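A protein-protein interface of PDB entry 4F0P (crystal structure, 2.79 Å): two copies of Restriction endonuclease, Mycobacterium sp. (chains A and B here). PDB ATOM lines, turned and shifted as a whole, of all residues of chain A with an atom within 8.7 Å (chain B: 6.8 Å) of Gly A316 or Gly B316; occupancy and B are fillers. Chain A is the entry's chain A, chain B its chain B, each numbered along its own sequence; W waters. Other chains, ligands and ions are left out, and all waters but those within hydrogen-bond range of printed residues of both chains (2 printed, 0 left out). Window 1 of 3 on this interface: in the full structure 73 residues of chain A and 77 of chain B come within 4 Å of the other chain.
Ser A315 touches Gly B316, and with the chains exchanged Gly A316 touches Ser B315.
Ser A315 touches Ala B317, and with the chains exchanged Ala A317 touches Ser B315.
Ser A315 touches Arg B318, and with the chains exchanged Arg A318 touches Ser B315.
Ser A315 touches Gly B342, and with the chains exchanged Gly A342 touches Ser B315.
Of the 20 pairs that touch across the chains among the printed residues, 12 have their exchanged pair printed and touching as well.
The backbone NH (N) of Glu A185 lies within hydrogen-bond range of the backbone carbonyl oxygen (O) of Asp A207, 2.8 Å away.
The backbone carbonyl oxygen (O) of Arg A318 sits at hydrogen-bond distance from the backbone NH (N) of Asp A340, at 2.9 Å.
A ring nitrogen (NE2) of His A111 is in hydrogen-bond range of the side-chain carboxylate (OD2) of Asp A207, 3.4 Å away.
The guanidinium group of Arg A186 sits at hydrogen-bond distance from the backbone carbonyl oxygen of Ser A315, 2.9 Å away.
The backbone NH (N) of Ala B317 sits at hydrogen-bond distance from the backbone carbonyl oxygen (O) of Phe B312 (3.0 Å).
O of Val B311 sits at hydrogen-bond distance from OG of Ser B315 (3.2 Å).
Glu A310 touches none of the printed residues of chain B.
Gly A316 touches two residues of chain B.
Of the printed residues of chain A, Arg B313 touches Arg A253 (3.4 Å).
Of the printed residues of chain A, Glu B314 touches Leu A344.
Of chain A, only Gly A316 (3.4 Å), Ala A317 (3.5 Å), Arg A318 (3.7 Å), Met A341 (3.8 Å) and Gly A342 (2.7 Å) come within 4 Å of Ser B315.
Of chain A, only Ser A315 and Gly A316 come within 4 Å of Gly B316.
Ala B317 touches just one residue of chain A: Ser A315 (3.8 Å).
Water W1 lies within hydrogen-bond range of OG of Ser A315 (2.7 Å) and N of Arg B318 (3.1 Å).
Water W2 bridges the backbone NH of Gly B342 (3.0 Å) and the backbone carbonyl oxygen of Phe A312 (3.2 Å).
Among the printed residues, merely in contact across the chains: Arg A253 with Arg B313 (3.4 Å), Val A311 with Gly B342 (3.6 Å), Phe A312 with Gly B342 (3.9 Å), Ser A315 with Ala B317 (3.8 Å), Ser A315 with Arg B318 (3.9 Å), Ser A315 with Gly B342 (3.5 Å), Gly A316 with Gly B316 (3.7 Å), Ala A317 with Ser B315 (3.5 Å), Arg A318 with Ser B315 (3.7 Å), Met A341 with Phe B312 (3.6 Å), Met A341 with Ser B315 (3.8 Å), Gly A342 with Val B311 (3.8 Å) and Leu A344 with Glu B314 (3.3 Å).
Of the 12 printed residues of chain B, 10 touch a printed residue of chain A.
Printed residues of chain B that touch a printed residue of chain A: Arg B186, Val B311, Phe B312, Arg B313, Glu B314, Ser B315, Gly B316, Ala B317, Arg B318 and Gly B342.
Hydrophobic or aromatic side chains of chain B that line the printed part of chain A: Val B311 and Phe B312.
Along chain B the printed residues that touch a printed residue of chain A span positions 186 to 342.
Hydrophobic or aromatic side chains of chain A within 4 Å of the printed part of chain B: His A111, Phe A312, Met A341 and Leu A344.
Among the printed residues, 20 pairs touch across the chains.
O of Gly B316 sits at hydrogen-bond distance from OG of Ser A315 (2.5 Å).
OE1 of Glu A185 is in salt-bridge range of NH1 of Arg B318, 3.1 Å away.
The side-chain carboxylate (OE2) of Glu A188 is in salt-bridge range of the guanidinium group (NH1) of Arg B186 (3.9 Å).
NE2 of His A111 is in hydrogen-bond range of NH1 of Arg B318 (3.2 Å).
N of Gly A342 lies within hydrogen-bond range of OG of Ser B315 (2.7 Å).
O of Gly A316 sits close to O of Ser B315.
The guanidinium group (NH1) of Arg A186 lies close to the guanidinium group (NH1) of Arg B186 (3.2 Å).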
ATOM      1  N   HIS A 111      17.913   7.160  13.331  1.00  0.00           N
ATOM      2  CA  HIS A 111      17.257   6.667  14.535  1.00  0.00           C
ATOM      3  C   HIS A 111      16.622   7.819  15.311  1.00  0.00           C
ATOM      4  O   HIS A 111      17.261   8.844  15.552  1.00  0.00           O
ATOM      5  CB  HIS A 111      18.264   5.924  15.414  1.00  0.00           C
ATOM      6  CG  HIS A 111      17.636   5.157  16.536  1.00  0.00           C
ATOM      7  ND1 HIS A 111      18.356   4.703  17.621  1.00  0.00           N
ATOM      8  CD2 HIS A 111      16.358   4.759  16.740  1.00  0.00           C
ATOM      9  CE1 HIS A 111      17.548   4.063  18.446  1.00  0.00           C
ATOM     10  NE2 HIS A 111      16.330   4.082  17.935  1.00  0.00           N
ATOM     11  N   ARG A 113      14.209   8.548  18.846  1.00  0.00           N
ATOM     12  CA  ARG A 113      13.450   8.168  20.032  1.00  0.00           C
ATOM     13  C   ARG A 113      12.361   9.208  20.272  1.00  0.00           C
ATOM     14  O   ARG A 113      12.657  10.358  20.611  1.00  0.00           O
ATOM     15  CB  ARG A 113      14.365   8.075  21.256  1.00  0.00           C
ATOM     16  CG  ARG A 113      15.462   7.024  21.149  1.00  0.00           C
ATOM     17  CD  ARG A 113      14.997   5.672  21.670  1.00  0.00           C
ATOM     18  NE  ARG A 113      14.803   5.682  23.117  1.00  0.00           N
ATOM     19  CZ  ARG A 113      14.323   4.656  23.814  1.00  0.00           C
ATOM     20  NH1 ARG A 113      14.181   4.753  25.129  1.00  0.00           N
ATOM     21  NH2 ARG A 113      13.985   3.532  23.197  1.00  0.00           N
ATOM     22  N   GLU A 185       9.994   1.193  14.248  1.00  0.00           N
ATOM     23  CA  GLU A 185      10.724  -0.016  14.623  1.00  0.00           C
ATOM     24  C   GLU A 185      10.093  -0.646  15.852  1.00  0.00           C
ATOM     25  O   GLU A 185       9.747  -1.828  15.849  1.00  0.00           O
ATOM     26  CB  GLU A 185      12.192   0.286  14.938  1.00  0.00           C
ATOM     27  CG  GLU A 185      13.052   0.689  13.758  1.00  0.00           C
ATOM     28  CD  GLU A 185      14.511   0.876  14.150  1.00  0.00           C
ATOM     29  OE1 GLU A 185      15.013   2.020  14.084  1.00  0.00           O
ATOM     30  OE2 GLU A 185      15.156  -0.125  14.526  1.00  0.00           O
ATOM     31  N   ARG A 186       9.955   0.145  16.914  1.00  0.00           N
ATOM     32  CA  ARG A 186       9.478  -0.404  18.181  1.00  0.00           C
ATOM     33  C   ARG A 186       8.519   0.541  18.902  1.00  0.00           C
ATOM     34  O   ARG A 186       8.633   1.760  18.793  1.00  0.00           O
ATOM     35  CB  ARG A 186      10.668  -0.755  19.086  1.00  0.00           C
ATOM     36  CG  ARG A 186      10.325  -1.640  20.274  1.00  0.00           C
ATOM     37  CD  ARG A 186      11.570  -2.020  21.066  1.00  0.00           C
ATOM     38  NE  ARG A 186      12.239  -0.853  21.633  1.00  0.00           N
ATOM     39  CZ  ARG A 186      13.308  -0.912  22.423  1.00  0.00           C
ATOM     40  NH1 ARG A 186      13.831  -2.086  22.747  1.00  0.00           N
ATOM     41  NH2 ARG A 186      13.851   0.203  22.893  1.00  0.00           N
ATOM     42  N   GLU A 188       6.779   0.689  22.853  1.00  0.00           N
ATOM     43  CA  GLU A 188       6.673   0.059  24.164  1.00  0.00           C
ATOM     44  C   GLU A 188       5.977   0.952  25.181  1.00  0.00           C
ATOM     45  O   GLU A 188       5.911   2.169  25.017  1.00  0.00           O
ATOM     46  CB  GLU A 188       8.055  -0.339  24.686  1.00  0.00           C
ATOM     47  CG  GLU A 188       8.888   0.828  25.182  1.00  0.00           C
ATOM     48  CD  GLU A 188      10.204   0.389  25.792  1.00  0.00           C
ATOM     49  OE1 GLU A 188      10.882   1.232  26.418  1.00  0.00           O
ATOM     50  OE2 GLU A 188      10.561  -0.798  25.645  1.00  0.00           O
ATOM     51  N   ASP A 207      10.700   3.748  19.041  1.00  0.00           N
ATOM     52  CA  ASP A 207      11.941   3.747  18.281  1.00  0.00           C
ATOM     53  C   ASP A 207      11.593   3.799  16.797  1.00  0.00           C
ATOM     54  O   ASP A 207      10.968   2.873  16.262  1.00  0.00           O
ATOM     55  CB  ASP A 207      12.762   2.492  18.586  1.00  0.00           C
ATOM     56  CG  ASP A 207      13.193   2.414  20.039  1.00  0.00           C
ATOM     57  OD1 ASP A 207      12.362   2.028  20.889  1.00  0.00           O
ATOM     58  OD2 ASP A 207      14.366   2.732  20.328  1.00  0.00           O
ATOM     59  N   ARG A 253      10.131  -6.341   7.912  1.00  0.00           N
ATOM     60  CA  ARG A 253      11.086  -6.038   8.973  1.00  0.00           C
ATOM     61  C   ARG A 253      12.517  -6.365   8.546  1.00  0.00           C
ATOM     62  O   ARG A 253      13.480  -5.863   9.126  1.00  0.00           O
ATOM     63  CB  ARG A 253      10.721  -6.807  10.249  1.00  0.00           C
ATOM     64  CG  ARG A 253      11.492  -6.378  11.492  1.00  0.00           C
ATOM     65  CD  ARG A 253      11.122  -7.224  12.706  1.00  0.00           C
ATOM     66  NE  ARG A 253      11.935  -6.891  13.874  1.00  0.00           N
ATOM     67  CZ  ARG A 253      11.853  -7.513  15.048  1.00  0.00           C
ATOM     68  NH1 ARG A 253      10.991  -8.506  15.215  1.00  0.00           N
ATOM     69  NH2 ARG A 253      12.633  -7.142  16.054  1.00  0.00           N
ATOM     70  N   ALA A 309      24.353   0.598  33.384  1.00  0.00           N
ATOM     71  CA  ALA A 309      23.256  -0.356  33.258  1.00  0.00           C
ATOM     72  C   ALA A 309      22.078   0.247  32.495  1.00  0.00           C
ATOM     73  O   ALA A 309      21.578  -0.351  31.546  1.00  0.00           O
ATOM     74  CB  ALA A 309      22.813  -0.847  34.628  1.00  0.00           C
ATOM     75  N   GLU A 310      21.653   1.441  32.901  1.00  0.00           N
ATOM     76  CA  GLU A 310      20.523   2.108  32.254  1.00  0.00           C
ATOM     77  C   GLU A 310      20.796   2.407  30.778  1.00  0.00           C
ATOM     78  O   GLU A 310      19.944   2.171  29.910  1.00  0.00           O
ATOM     79  CB  GLU A 310      20.172   3.400  32.993  1.00  0.00           C
ATOM     80  CG  GLU A 310      18.807   3.963  32.636  1.00  0.00           C
ATOM     81  CD  GLU A 310      17.678   3.019  33.004  1.00  0.00           C
ATOM     82  OE1 GLU A 310      17.830   2.259  33.986  1.00  0.00           O
ATOM     83  OE2 GLU A 310      16.641   3.031  32.307  1.00  0.00           O
ATOM     84  N   VAL A 311      21.993   2.922  30.506  1.00  0.00           N
ATOM     85  CA  VAL A 311      22.412   3.257  29.148  1.00  0.00           C
ATOM     86  C   VAL A 311      22.390   2.040  28.224  1.00  0.00           C
ATOM     87  O   VAL A 311      21.917   2.124  27.089  1.00  0.00           O
ATOM     88  CB  VAL A 311      23.812   3.916  29.138  1.00  0.00           C
ATOM     89  CG1 VAL A 311      24.434   3.857  27.752  1.00  0.00           C
ATOM     90  CG2 VAL A 311      23.721   5.352  29.627  1.00  0.00           C
ATOM     91  N   PHE A 312      22.888   0.907  28.713  1.00  0.00           N
ATOM     92  CA  PHE A 312      22.841  -0.326  27.928  1.00  0.00           C
ATOM     93  C   PHE A 312      21.423  -0.884  27.801  1.00  0.00           C
ATOM     94  O   PHE A 312      21.075  -1.490  26.786  1.00  0.00           O
ATOM     95  CB  PHE A 312      23.778  -1.387  28.509  1.00  0.00           C
ATOM     96  CG  PHE A 312      25.214  -1.200  28.120  1.00  0.00           C
ATOM     97  CD1 PHE A 312      25.626  -1.443  26.820  1.00  0.00           C
ATOM     98  CD2 PHE A 312      26.152  -0.783  29.048  1.00  0.00           C
ATOM     99  CE1 PHE A 312      26.947  -1.271  26.453  1.00  0.00           C
ATOM    100  CE2 PHE A 312      27.475  -0.610  28.687  1.00  0.00           C
ATOM    101  CZ  PHE A 312      27.873  -0.854  27.387  1.00  0.00           C
ATOM    102  N   ARG A 313      20.608  -0.673  28.830  1.00  0.00           N
ATOM    103  CA  ARG A 313      19.239  -1.182  28.835  1.00  0.00           C
ATOM    104  C   ARG A 313      18.288  -0.358  27.968  1.00  0.00           C
ATOM    105  O   ARG A 313      17.180  -0.808  27.673  1.00  0.00           O
ATOM    106  CB  ARG A 313      18.692  -1.280  30.262  1.00  0.00           C
ATOM    107  CG  ARG A 313      19.296  -2.403  31.092  1.00  0.00           C
ATOM    108  CD  ARG A 313      18.688  -2.435  32.487  1.00  0.00           C
ATOM    109  NE  ARG A 313      17.374  -3.074  32.499  1.00  0.00           N
ATOM    110  CZ  ARG A 313      16.467  -2.900  33.454  1.00  0.00           C
ATOM    111  NH1 ARG A 313      16.720  -2.092  34.476  1.00  0.00           N
ATOM    112  NH2 ARG A 313      15.301  -3.525  33.382  1.00  0.00           N
ATOM    113  N   GLU A 314      18.708   0.844  27.572  1.00  0.00           N
ATOM    114  CA  GLU A 314      17.886   1.666  26.679  1.00  0.00           C
ATOM    115  C   GLU A 314      17.530   0.933  25.388  1.00  0.00           C
ATOM    116  O   GLU A 314      16.381   0.966  24.938  1.00  0.00           O
ATOM    117  CB  GLU A 314      18.573   2.991  26.337  1.00  0.00           C
ATOM    118  CG  GLU A 314      18.007   3.638  25.074  1.00  0.00           C
ATOM    119  CD  GLU A 314      18.359   5.104  24.940  1.00  0.00           C
ATOM    120  OE1 GLU A 314      18.723   5.727  25.960  1.00  0.00           O
ATOM    121  OE2 GLU A 314      18.271   5.635  23.812  1.00  0.00           O
ATOM    122  N   SER A 315      18.522   0.270  24.801  1.00  0.00           N
ATOM    123  CA  SER A 315      18.329  -0.478  23.562  1.00  0.00           C
ATOM    124  C   SER A 315      17.344  -1.633  23.741  1.00  0.00           C
ATOM    125  O   SER A 315      16.729  -2.092  22.778  1.00  0.00           O
ATOM    126  CB  SER A 315      19.673  -1.003  23.050  1.00  0.00           C
ATOM    127  OG  SER A 315      19.511  -1.777  21.873  1.00  0.00           O
ATOM    128  N   GLY A 316      17.189  -2.090  24.979  1.00  0.00           N
ATOM    129  CA  GLY A 316      16.351  -3.237  25.273  1.00  0.00           C
ATOM    130  C   GLY A 316      17.220  -4.468  25.417  1.00  0.00           C
ATOM    131  O   GLY A 316      16.728  -5.595  25.450  1.00  0.00           O
ATOM    132  N   ALA A 317      18.526  -4.234  25.505  1.00  0.00           N
ATOM    133  CA  ALA A 317      19.509  -5.307  25.588  1.00  0.00           C
ATOM    134  C   ALA A 317      19.394  -6.095  26.888  1.00  0.00           C
ATOM    135  O   ALA A 317      18.811  -5.627  27.869  1.00  0.00           O
ATOM    136  CB  ALA A 317      20.917  -4.745  25.430  1.00  0.00           C
ATOM    137  N   ARG A 318      19.954  -7.299  26.882  1.00  0.00           N
ATOM    138  CA  ARG A 318      19.938  -8.167  28.049  1.00  0.00           C
ATOM    139  C   ARG A 318      21.150  -7.885  28.930  1.00  0.00           C
ATOM    140  O   ARG A 318      22.189  -8.531  28.799  1.00  0.00           O
ATOM    141  CB  ARG A 318      19.939  -9.630  27.606  1.00  0.00           C
ATOM    142  CG  ARG A 318      19.815 -10.626  28.741  1.00  0.00           C
ATOM    143  CD  ARG A 318      18.435 -10.588  29.357  1.00  0.00           C
ATOM    144  NE  ARG A 318      18.291 -11.593  30.402  1.00  0.00           N
ATOM    145  CZ  ARG A 318      17.128 -11.950  30.935  1.00  0.00           C
ATOM    146  NH1 ARG A 318      16.008 -11.381  30.512  1.00  0.00           N
ATOM    147  NH2 ARG A 318      17.088 -12.876  31.883  1.00  0.00           N
ATOM    148  N   TYR A 319      21.018  -6.911  29.824  1.00  0.00           N
ATOM    149  CA  TYR A 319      22.125  -6.520  30.690  1.00  0.00           C
ATOM    150  C   TYR A 319      21.972  -7.080  32.101  1.00  0.00           C
ATOM    151  O   TYR A 319      20.882  -7.067  32.673  1.00  0.00           O
ATOM    152  CB  TYR A 319      22.259  -4.994  30.741  1.00  0.00           C
ATOM    153  CG  TYR A 319      23.492  -4.509  31.475  1.00  0.00           C
ATOM    154  CD1 TYR A 319      23.466  -4.279  32.846  1.00  0.00           C
ATOM    155  CD2 TYR A 319      24.682  -4.278  30.796  1.00  0.00           C
ATOM    156  CE1 TYR A 319      24.593  -3.838  33.521  1.00  0.00           C
ATOM    157  CE2 TYR A 319      25.813  -3.836  31.461  1.00  0.00           C
ATOM    158  CZ  TYR A 319      25.762  -3.616  32.824  1.00  0.00           C
ATOM    159  OH  TYR A 319      26.883  -3.174  33.492  1.00  0.00           O
ATOM    160  N   ILE A 339      26.543  -8.587  29.307  1.00  0.00           N
ATOM    161  CA  ILE A 339      25.464  -8.441  28.335  1.00  0.00           C
ATOM    162  C   ILE A 339      25.241  -9.740  27.570  1.00  0.00           C
ATOM    163  O   ILE A 339      26.047 -10.113  26.721  1.00  0.00           O
ATOM    164  CB  ILE A 339      25.767  -7.327  27.311  1.00  0.00           C
ATOM    165  CG1 ILE A 339      25.991  -5.990  28.017  1.00  0.00           C
ATOM    166  CG2 ILE A 339      24.639  -7.210  26.295  1.00  0.00           C
ATOM    167  CD1 ILE A 339      26.342  -4.861  27.078  1.00  0.00           C
ATOM    168  N   ASP A 340      24.145 -10.426  27.868  1.00  0.00           N
ATOM    169  CA  ASP A 340      23.822 -11.665  27.170  1.00  0.00           C
ATOM    170  C   ASP A 340      23.326 -11.365  25.757  1.00  0.00           C
ATOM    171  O   ASP A 340      22.394 -10.582  25.567  1.00  0.00           O
ATOM    172  CB  ASP A 340      22.783 -12.462  27.955  1.00  0.00           C
ATOM    173  CG  ASP A 340      23.168 -12.633  29.411  1.00  0.00           C
ATOM    174  OD1 ASP A 340      24.374 -12.802  29.691  1.00  0.00           O
ATOM    175  OD2 ASP A 340      22.267 -12.588  30.275  1.00  0.00           O
ATOM    176  N   MET A 341      23.957 -11.994  24.769  1.00  0.00           N
ATOM    177  CA  MET A 341      23.678 -11.699  23.368  1.00  0.00           C
ATOM    178  C   MET A 341      23.252 -12.941  22.593  1.00  0.00           C
ATOM    179  O   MET A 341      24.005 -13.910  22.505  1.00  0.00           O
ATOM    180  CB  MET A 341      24.921 -11.107  22.705  1.00  0.00           C
ATOM    181  CG  MET A 341      24.643 -10.384  21.405  1.00  0.00           C
ATOM    182  SD  MET A 341      24.467  -8.615  21.684  1.00  0.00           S
ATOM    183  CE  MET A 341      26.036  -8.281  22.473  1.00  0.00           C
ATOM    184  N   GLY A 342      22.052 -12.907  22.023  1.00  0.00           N
ATOM    185  CA  GLY A 342      21.587 -14.000  21.190  1.00  0.00           C
ATOM    186  C   GLY A 342      20.268 -14.601  21.633  1.00  0.00           C
ATOM    187  O   GLY A 342      19.441 -13.935  22.260  1.00  0.00           O
ATOM    188  N   LEU A 344      17.530 -16.863  23.659  1.00  0.00           N
ATOM    189  CA  LEU A 344      17.312 -17.102  25.079  1.00  0.00           C
ATOM    190  C   LEU A 344      17.812 -18.492  25.466  1.00  0.00           C
ATOM    191  O   LEU A 344      18.210 -18.724  26.608  1.00  0.00           O
ATOM    192  CB  LEU A 344      15.832 -16.940  25.438  1.00  0.00           C
ATOM    193  CG  LEU A 344      15.341 -15.522  25.752  1.00  0.00           C
ATOM    194  CD1 LEU A 344      16.140 -14.923  26.901  1.00  0.00           C
ATOM    195  CD2 LEU A 344      15.394 -14.616  24.525  1.00  0.00           C
ATOM    196  N   ARG B 186       9.527  -5.395  30.706  1.00  0.00           N
ATOM    197  CA  ARG B 186       9.168  -4.676  29.491  1.00  0.00           C
ATOM    198  C   ARG B 186       7.768  -5.026  29.005  1.00  0.00           C
ATOM    199  O   ARG B 186       7.335  -6.171  29.102  1.00  0.00           O
ATOM    200  CB  ARG B 186      10.203  -4.936  28.392  1.00  0.00           C
ATOM    201  CG  ARG B 186      10.173  -3.930  27.252  1.00  0.00           C
ATOM    202  CD  ARG B 186      11.566  -3.706  26.677  1.00  0.00           C
ATOM    203  NE  ARG B 186      12.101  -4.901  26.029  1.00  0.00           N
ATOM    204  CZ  ARG B 186      12.139  -5.082  24.712  1.00  0.00           C
ATOM    205  NH1 ARG B 186      11.677  -4.142  23.898  1.00  0.00           N
ATOM    206  NH2 ARG B 186      12.643  -6.200  24.207  1.00  0.00           N
ATOM    207  N   ASP B 207       8.380  -8.808  28.561  1.00  0.00           N
ATOM    208  CA  ASP B 207       9.595  -9.383  29.117  1.00  0.00           C
ATOM    209  C   ASP B 207       9.489  -9.364  30.637  1.00  0.00           C
ATOM    210  O   ASP B 207       9.478  -8.294  31.258  1.00  0.00           O
ATOM    211  CB  ASP B 207      10.824  -8.600  28.660  1.00  0.00           C
ATOM    212  CG  ASP B 207      11.017  -8.648  27.161  1.00  0.00           C
ATOM    213  OD1 ASP B 207      10.625  -9.661  26.546  1.00  0.00           O
ATOM    214  OD2 ASP B 207      11.559  -7.674  26.598  1.00  0.00           O
ATOM    215  N   VAL B 311      17.735 -12.463  15.211  1.00  0.00           N
ATOM    216  CA  VAL B 311      18.128 -12.919  16.546  1.00  0.00           C
ATOM    217  C   VAL B 311      18.717 -11.777  17.374  1.00  0.00           C
ATOM    218  O   VAL B 311      18.385 -11.609  18.553  1.00  0.00           O
ATOM    219  CB  VAL B 311      19.139 -14.083  16.480  1.00  0.00           C
ATOM    220  CG1 VAL B 311      19.696 -14.392  17.865  1.00  0.00           C
ATOM    221  CG2 VAL B 311      18.489 -15.318  15.873  1.00  0.00           C
ATOM    222  N   PHE B 312      19.586 -10.987  16.749  1.00  0.00           N
ATOM    223  CA  PHE B 312      20.161  -9.827  17.422  1.00  0.00           C
ATOM    224  C   PHE B 312      19.097  -8.785  17.747  1.00  0.00           C
ATOM    225  O   PHE B 312      19.236  -8.026  18.707  1.00  0.00           O
ATOM    226  CB  PHE B 312      21.281  -9.212  16.587  1.00  0.00           C
ATOM    227  CG  PHE B 312      22.561  -9.994  16.628  1.00  0.00           C
ATOM    228  CD1 PHE B 312      23.077 -10.434  17.836  1.00  0.00           C
ATOM    229  CD2 PHE B 312      23.238 -10.305  15.462  1.00  0.00           C
ATOM    230  CE1 PHE B 312      24.254 -11.158  17.881  1.00  0.00           C
ATOM    231  CE2 PHE B 312      24.415 -11.030  15.500  1.00  0.00           C
ATOM    232  CZ  PHE B 312      24.923 -11.458  16.713  1.00  0.00           C
ATOM    233  N   ARG B 313      18.036  -8.749  16.948  1.00  0.00           N
ATOM    234  CA  ARG B 313      16.903  -7.878  17.245  1.00  0.00           C
ATOM    235  C   ARG B 313      16.122  -8.419  18.442  1.00  0.00           C
ATOM    236  O   ARG B 313      15.612  -7.652  19.259  1.00  0.00           O
ATOM    237  CB  ARG B 313      15.988  -7.734  16.028  1.00  0.00           C
ATOM    238  N   GLU B 314      16.035  -9.743  18.536  1.00  0.00           N
ATOM    239  CA  GLU B 314      15.397 -10.404  19.670  1.00  0.00           C
ATOM    240  C   GLU B 314      16.155 -10.088  20.954  1.00  0.00           C
ATOM    241  O   GLU B 314      15.551  -9.886  22.009  1.00  0.00           O
ATOM    242  CB  GLU B 314      15.341 -11.919  19.446  1.00  0.00           C
ATOM    243  CG  GLU B 314      15.090 -12.745  20.706  1.00  0.00           C
ATOM    244  CD  GLU B 314      13.663 -12.638  21.212  1.00  0.00           C
ATOM    245  OE1 GLU B 314      12.784 -12.216  20.432  1.00  0.00           O
ATOM    246  OE2 GLU B 314      13.422 -12.980  22.390  1.00  0.00           O
ATOM    247  N   SER B 315      17.481 -10.037  20.853  1.00  0.00           N
ATOM    248  CA  SER B 315      18.322  -9.704  21.998  1.00  0.00           C
ATOM    249  C   SER B 315      18.098  -8.269  22.469  1.00  0.00           C
ATOM    250  O   SER B 315      18.338  -7.944  23.631  1.00  0.00           O
ATOM    251  CB  SER B 315      19.797  -9.915  21.657  1.00  0.00           C
ATOM    252  OG  SER B 315      20.043 -11.266  21.314  1.00  0.00           O
ATOM    253  N   GLY B 316      17.638  -7.417  21.560  1.00  0.00           N
ATOM    254  CA  GLY B 316      17.386  -6.022  21.874  1.00  0.00           C
ATOM    255  C   GLY B 316      18.406  -5.101  21.234  1.00  0.00           C
ATOM    256  O   GLY B 316      18.260  -3.879  21.264  1.00  0.00           O
ATOM    257  N   ALA B 317      19.441  -5.690  20.646  1.00  0.00           N
ATOM    258  CA  ALA B 317      20.511  -4.919  20.026  1.00  0.00           C
ATOM    259  C   ALA B 317      20.075  -4.293  18.702  1.00  0.00           C
ATOM    260  O   ALA B 317      19.244  -4.851  17.985  1.00  0.00           O
ATOM    261  CB  ALA B 317      21.736  -5.796  19.822  1.00  0.00           C
ATOM    262  N   ARG B 318      20.639  -3.129  18.388  1.00  0.00           N
ATOM    263  CA  ARG B 318      20.375  -2.466  17.114  1.00  0.00           C
ATOM    264  C   ARG B 318      21.334  -2.961  16.037  1.00  0.00           C
ATOM    265  O   ARG B 318      22.512  -2.602  16.022  1.00  0.00           O
ATOM    266  CB  ARG B 318      20.475  -0.947  17.256  1.00  0.00           C
ATOM    267  CG  ARG B 318      19.247  -0.305  17.875  1.00  0.00           C
ATOM    268  CD  ARG B 318      19.394   1.205  17.953  1.00  0.00           C
ATOM    269  NE  ARG B 318      19.687   1.805  16.654  1.00  0.00           N
ATOM    270  CZ  ARG B 318      18.766   2.114  15.745  1.00  0.00           C
ATOM    271  NH1 ARG B 318      17.485   1.872  15.988  1.00  0.00           N
ATOM    272  NH2 ARG B 318      19.126   2.662  14.591  1.00  0.00           N
ATOM    273  N   TYR B 319      20.815  -3.783  15.133  1.00  0.00           N
ATOM    274  CA  TYR B 319      21.627  -4.416  14.102  1.00  0.00           C
ATOM    275  C   TYR B 319      21.632  -3.597  12.812  1.00  0.00           C
ATOM    276  O   TYR B 319      20.655  -2.917  12.491  1.00  0.00           O
ATOM    277  CB  TYR B 319      21.112  -5.833  13.838  1.00  0.00           C
ATOM    278  CG  TYR B 319      21.935  -6.639  12.861  1.00  0.00           C
ATOM    279  CD1 TYR B 319      23.013  -7.402  13.296  1.00  0.00           C
ATOM    280  CD2 TYR B 319      21.628  -6.649  11.508  1.00  0.00           C
ATOM    281  CE1 TYR B 319      23.767  -8.147  12.403  1.00  0.00           C
ATOM    282  CE2 TYR B 319      22.375  -7.390  10.608  1.00  0.00           C
ATOM    283  CZ  TYR B 319      23.442  -8.137  11.060  1.00  0.00           C
ATOM    284  OH  TYR B 319      24.184  -8.872  10.163  1.00  0.00           O
ATOM    285  N   GLY B 342      24.920   0.079  23.239  1.00  0.00           N
ATOM    286  CA  GLY B 342      24.726   1.223  24.107  1.00  0.00           C
ATOM    287  C   GLY B 342      23.383   1.878  23.859  1.00  0.00           C
ATOM    288  O   GLY B 342      22.411   1.209  23.500  1.00  0.00           O
HETATM  289  O   HOH W   1      22.032  -2.138  20.945  1.00  0.00           O
HETATM  290  O   HOH W   2      22.827  -1.860  24.184  1.00  0.00           O
